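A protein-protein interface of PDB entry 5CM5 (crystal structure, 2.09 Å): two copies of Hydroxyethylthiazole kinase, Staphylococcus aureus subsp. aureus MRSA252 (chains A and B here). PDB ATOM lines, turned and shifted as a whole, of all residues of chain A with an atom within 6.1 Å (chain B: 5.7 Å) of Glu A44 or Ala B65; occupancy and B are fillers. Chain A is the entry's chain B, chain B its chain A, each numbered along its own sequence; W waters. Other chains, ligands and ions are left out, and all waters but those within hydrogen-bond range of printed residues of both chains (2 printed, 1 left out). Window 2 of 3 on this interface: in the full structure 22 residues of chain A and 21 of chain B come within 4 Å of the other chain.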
ATOM      1  N   GLU A  41      19.249 -27.033  13.373  1.00  0.00           N
ATOM      2  CA  GLU A  41      18.570 -27.647  14.494  1.00  0.00           C
ATOM      3  C   GLU A  41      17.397 -26.858  15.103  1.00  0.00           C
ATOM      4  O   GLU A  41      16.743 -27.355  16.016  1.00  0.00           O
ATOM      5  CB  GLU A  41      19.590 -27.975  15.585  1.00  0.00           C
ATOM      6  CG  GLU A  41      20.700 -28.970  15.108  1.00  0.00           C
ATOM      7  CD  GLU A  41      21.815 -29.153  16.122  1.00  0.00           C
ATOM      8  OE1 GLU A  41      21.558 -28.939  17.325  1.00  0.00           O
ATOM      9  OE2 GLU A  41      22.962 -29.531  15.705  1.00  0.00           O
ATOM     10  N   ALA A  42      17.181 -25.652  14.616  1.00  0.00           N
ATOM     11  CA  ALA A  42      16.056 -24.788  15.092  1.00  0.00           C
ATOM     12  C   ALA A  42      14.795 -25.099  14.373  1.00  0.00           C
ATOM     13  O   ALA A  42      14.697 -24.948  13.154  1.00  0.00           O
ATOM     14  CB  ALA A  42      16.418 -23.342  14.879  1.00  0.00           C
ATOM     15  N   PRO A  43      13.787 -25.564  15.102  1.00  0.00           N
ATOM     16  CA  PRO A  43      12.424 -25.681  14.511  1.00  0.00           C
ATOM     17  C   PRO A  43      11.926 -24.414  13.784  1.00  0.00           C
ATOM     18  O   PRO A  43      11.153 -24.524  12.856  1.00  0.00           O
ATOM     19  CB  PRO A  43      11.514 -25.970  15.714  1.00  0.00           C
ATOM     20  CG  PRO A  43      12.441 -26.569  16.745  1.00  0.00           C
ATOM     21  CD  PRO A  43      13.795 -25.928  16.528  1.00  0.00           C
ATOM     22  N   GLU A  44      12.423 -23.270  14.212  1.00  0.00           N
ATOM     23  CA  GLU A  44      11.911 -21.930  13.735  1.00  0.00           C
ATOM     24  C   GLU A  44      12.316 -21.705  12.285  1.00  0.00           C
ATOM     25  O   GLU A  44      11.706 -20.915  11.593  1.00  0.00           O
ATOM     26  CB  GLU A  44      12.473 -20.798  14.618  1.00  0.00           C
ATOM     27  CG  GLU A  44      12.011 -20.793  16.077  1.00  0.00           C
ATOM     28  CD  GLU A  44      12.844 -21.693  17.014  1.00  0.00           C
ATOM     29  OE1 GLU A  44      13.651 -22.567  16.567  1.00  0.00           O
ATOM     30  OE2 GLU A  44      12.711 -21.504  18.254  1.00  0.00           O
ATOM     31  N   GLU A  45      13.330 -22.428  11.796  1.00  0.00           N
ATOM     32  CA  GLU A  45      13.714 -22.264  10.385  1.00  0.00           C
ATOM     33  C   GLU A  45      13.433 -23.506   9.525  1.00  0.00           C
ATOM     34  O   GLU A  45      13.894 -23.615   8.372  1.00  0.00           O
ATOM     35  CB  GLU A  45      15.152 -21.789  10.282  1.00  0.00           C
ATOM     36  CG  GLU A  45      16.270 -22.843  10.622  1.00  0.00           C
ATOM     37  CD  GLU A  45      17.687 -22.259  10.595  1.00  0.00           C
ATOM     38  OE1 GLU A  45      17.872 -21.097  10.231  1.00  0.00           O
ATOM     39  OE2 GLU A  45      18.683 -23.020  10.943  1.00  0.00           O
ATOM     40  N   ALA A  46      12.801 -24.500  10.126  1.00  0.00           N
ATOM     41  CA  ALA A  46      12.683 -25.801   9.449  1.00  0.00           C
ATOM     42  C   ALA A  46      11.799 -25.704   8.221  1.00  0.00           C
ATOM     43  O   ALA A  46      12.116 -26.237   7.178  1.00  0.00           O
ATOM     44  CB  ALA A  46      12.154 -26.854  10.402  1.00  0.00           C
ATOM     45  N   GLU A  47      10.697 -24.949   8.327  1.00  0.00           N
ATOM     46  CA  GLU A  47       9.816 -24.744   7.225  1.00  0.00           C
ATOM     47  C   GLU A  47      10.556 -24.219   5.956  1.00  0.00           C
ATOM     48  O   GLU A  47      10.369 -24.722   4.861  1.00  0.00           O
ATOM     49  CB  GLU A  47       8.641 -23.793   7.692  1.00  0.00           C
ATOM     50  CG  GLU A  47       7.755 -24.182   8.899  1.00  0.00           C
ATOM     51  CD  GLU A  47       8.265 -23.556  10.242  1.00  0.00           C
ATOM     52  OE1 GLU A  47       9.537 -23.677  10.610  1.00  0.00           O
ATOM     53  OE2 GLU A  47       7.362 -22.855  10.881  1.00  0.00           O
ATOM     54  N   GLU A  48      11.368 -23.182   6.119  1.00  0.00           N
ATOM     55  CA  GLU A  48      12.026 -22.568   4.998  1.00  0.00           C
ATOM     56  C   GLU A  48      13.160 -23.470   4.495  1.00  0.00           C
ATOM     57  O   GLU A  48      13.369 -23.579   3.294  1.00  0.00           O
ATOM     58  CB  GLU A  48      12.583 -21.199   5.352  1.00  0.00           C
ATOM     59  CG  GLU A  48      11.504 -20.128   5.552  1.00  0.00           C
ATOM     60  CD  GLU A  48      12.106 -18.782   5.887  1.00  0.00           C
ATOM     61  OE1 GLU A  48      12.690 -18.606   6.958  1.00  0.00           O
ATOM     62  OE2 GLU A  48      12.061 -17.895   5.064  1.00  0.00           O
ATOM     63  N   LEU B  63      22.590 -21.822  15.129  1.00  0.00           N
ATOM     64  CA  LEU B  63      21.679 -21.024  15.938  1.00  0.00           C
ATOM     65  C   LEU B  63      20.418 -21.785  16.332  1.00  0.00           C
ATOM     66  O   LEU B  63      19.689 -22.276  15.468  1.00  0.00           O
ATOM     67  CB  LEU B  63      21.285 -19.748  15.144  1.00  0.00           C
ATOM     68  CG  LEU B  63      20.467 -18.686  15.859  1.00  0.00           C
ATOM     69  CD1 LEU B  63      21.276 -18.019  16.941  1.00  0.00           C
ATOM     70  CD2 LEU B  63      19.987 -17.625  14.857  1.00  0.00           C
ATOM     71  N   THR B  64      20.104 -21.766  17.623  1.00  0.00           N
ATOM     72  CA  THR B  64      18.805 -22.200  18.145  1.00  0.00           C
ATOM     73  C   THR B  64      18.303 -21.240  19.225  1.00  0.00           C
ATOM     74  O   THR B  64      19.040 -20.367  19.681  1.00  0.00           O
ATOM     75  CB  THR B  64      18.926 -23.623  18.765  1.00  0.00           C
ATOM     76  OG1 THR B  64      19.831 -23.578  19.878  1.00  0.00           O
ATOM     77  CG2 THR B  64      19.426 -24.657  17.723  1.00  0.00           C
ATOM     78  N   ALA B  65      17.053 -21.411  19.646  1.00  0.00           N
ATOM     79  CA  ALA B  65      16.434 -20.581  20.712  1.00  0.00           C
ATOM     80  C   ALA B  65      17.294 -20.480  21.964  1.00  0.00           C
ATOM     81  O   ALA B  65      17.403 -19.434  22.573  1.00  0.00           O
ATOM     82  CB  ALA B  65      15.065 -21.122  21.088  1.00  0.00           C
ATOM     83  N   GLN B  66      18.006 -21.563  22.280  1.00  0.00           N
ATOM     84  CA  GLN B  66      18.887 -21.594  23.433  1.00  0.00           C
ATOM     85  C   GLN B  66      20.121 -20.684  23.287  1.00  0.00           C
ATOM     86  O   GLN B  66      20.710 -20.295  24.277  1.00  0.00           O
ATOM     87  CB  GLN B  66      19.232 -23.073  23.754  1.00  0.00           C
ATOM     88  CG  GLN B  66      18.003 -23.846  24.327  1.00  0.00           C
ATOM     89  CD  GLN B  66      16.811 -24.045  23.340  1.00  0.00           C
ATOM     90  OE1 GLN B  66      16.987 -24.290  22.137  1.00  0.00           O
ATOM     91  NE2 GLN B  66      15.599 -24.011  23.877  1.00  0.00           N
ATOM     92  N   ASN B  67      20.544 -20.398  22.069  1.00  0.00           N
ATOM     93  CA  ASN B  67      21.707 -19.563  21.831  1.00  0.00           C
ATOM     94  C   ASN B  67      21.344 -18.047  21.837  1.00  0.00           C
ATOM     95  O   ASN B  67      22.217 -17.225  22.091  1.00  0.00           O
ATOM     96  CB  ASN B  67      22.296 -19.819  20.445  1.00  0.00           C
ATOM     97  CG  ASN B  67      22.852 -21.209  20.252  1.00  0.00           C
ATOM     98  OD1 ASN B  67      22.562 -21.855  19.257  1.00  0.00           O
ATOM     99  ND2 ASN B  67      23.697 -21.637  21.134  1.00  0.00           N
ATOM    100  N   GLU B  68      20.116 -17.709  21.434  1.00  0.00           N
ATOM    101  CA  GLU B  68      19.813 -16.335  21.018  1.00  0.00           C
ATOM    102  C   GLU B  68      20.105 -15.337  22.115  1.00  0.00           C
ATOM    103  O   GLU B  68      20.862 -14.395  21.884  1.00  0.00           O
ATOM    104  CB  GLU B  68      18.363 -16.190  20.555  1.00  0.00           C
ATOM    105  CG  GLU B  68      18.004 -16.952  19.266  1.00  0.00           C
ATOM    106  CD  GLU B  68      16.491 -17.020  19.062  1.00  0.00           C
ATOM    107  OE1 GLU B  68      15.858 -15.984  19.211  1.00  0.00           O
ATOM    108  OE2 GLU B  68      15.942 -18.077  18.730  1.00  0.00           O
ATOM    109  N   GLN B  69      19.596 -15.600  23.314  1.00  0.00           N
ATOM    110  CA  GLN B  69      19.807 -14.697  24.446  1.00  0.00           C
ATOM    111  C   GLN B  69      21.304 -14.637  24.823  1.00  0.00           C
ATOM    112  O   GLN B  69      21.843 -13.559  25.072  1.00  0.00           O
ATOM    113  CB  GLN B  69      19.090 -15.175  25.743  1.00  0.00           C
ATOM    114  CG  GLN B  69      18.997 -14.111  26.845  1.00  0.00           C
ATOM    115  CD  GLN B  69      18.119 -14.503  28.067  1.00  0.00           C
ATOM    116  OE1 GLN B  69      16.884 -14.301  28.076  1.00  0.00           O
ATOM    117  NE2 GLN B  69      18.763 -15.058  29.098  1.00  0.00           N
ATOM    118  N   TYR B  97      14.244 -16.534  10.159  1.00  0.00           N
ATOM    119  CA  TYR B  97      14.793 -16.727  11.507  1.00  0.00           C
ATOM    120  C   TYR B  97      16.190 -16.153  11.648  1.00  0.00           C
ATOM    121  O   TYR B  97      16.456 -15.387  12.592  1.00  0.00           O
ATOM    122  CB  TYR B  97      14.732 -18.209  11.891  1.00  0.00           C
ATOM    123  CG  TYR B  97      15.327 -18.556  13.230  1.00  0.00           C
ATOM    124  CD1 TYR B  97      14.787 -18.070  14.428  1.00  0.00           C
ATOM    125  CD2 TYR B  97      16.423 -19.400  13.309  1.00  0.00           C
ATOM    126  CE1 TYR B  97      15.359 -18.403  15.672  1.00  0.00           C
ATOM    127  CE2 TYR B  97      16.987 -19.747  14.524  1.00  0.00           C
ATOM    128  CZ  TYR B  97      16.449 -19.273  15.701  1.00  0.00           C
ATOM    129  OH  TYR B  97      17.062 -19.628  16.880  1.00  0.00           O
HETATM  130  O   HOH W   1      12.632 -19.228   9.291  1.00  0.00           O
HETATM  131  O   HOH W   2      19.557 -24.122  13.502  1.00  0.00           O
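CB of Glu A41 touches CG2 of Thr B64 (3.95 Å). Leu B63 touches Ala A42. Ala A42 touches Thr B64. Tyr B97 touches Ala A42 (CE2 to CB, 3.7 Å). OE2 of Glu A44 touches CB of Ala B65, 3.7 Å away. Glu A44 touches Tyr B97. Tyr B97 touches Glu A45.
No position is printed for both chains. Of the 7 pairs that touch across the chains among the printed residues, none has its exchanged pair printed and touching as well.
Water W1 lies within hydrogen-bond range of the side-chain carboxylate of Glu A48 (2.4 Å), the backbone carbonyl oxygen of Glu A44 (3.0 Å) and the backbone NH of Tyr B97 (3.3 Å). Water W2 lies within hydrogen-bond range of O of Leu B63 (2.7 Å), OE2 of Glu A45 (2.9 Å), N of Glu A41 (2.9 Å) and N of Ala A42 (3.0 Å).
N of Thr B64 is in hydrogen-bond range of OD1 of Asn B67 (3.0 Å). The side-chain hydroxyl (OH) of Tyr B97 is in hydrogen-bond range of the backbone NH (N) of Ala B65 (3.3 Å). The side-chain carboxylate of Glu B68 lies within hydrogen-bond range of the side-chain hydroxyl of Tyr B97 (2.7 Å).
Ala B65 touches just one residue of chain A: Glu A44. Of the printed residues of chain B, Ala A42 touches Leu B63, Thr B64 and Tyr B97. Of the printed residues of chain A, Tyr B97 touches Ala A42, Glu A44 and Glu A45. Of the printed residues of chain B, Glu A45 touches Tyr B97. Gln B66 touches none of the printed residues of chain A.
Hydrophobic or aromatic side chains of chain A within 4 Å of the printed part of chain B: Ala A42. Hydrophobic or aromatic side chains of chain B within 4 Å of the printed part of chain A: Ala B65 and Tyr B97. Among the printed residues, 7 pairs touch across the chains. Among the printed residues, no Asp or Glu carboxylate lies within 4 Å of a Lys or Arg side-chain nitrogen of the other chain.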
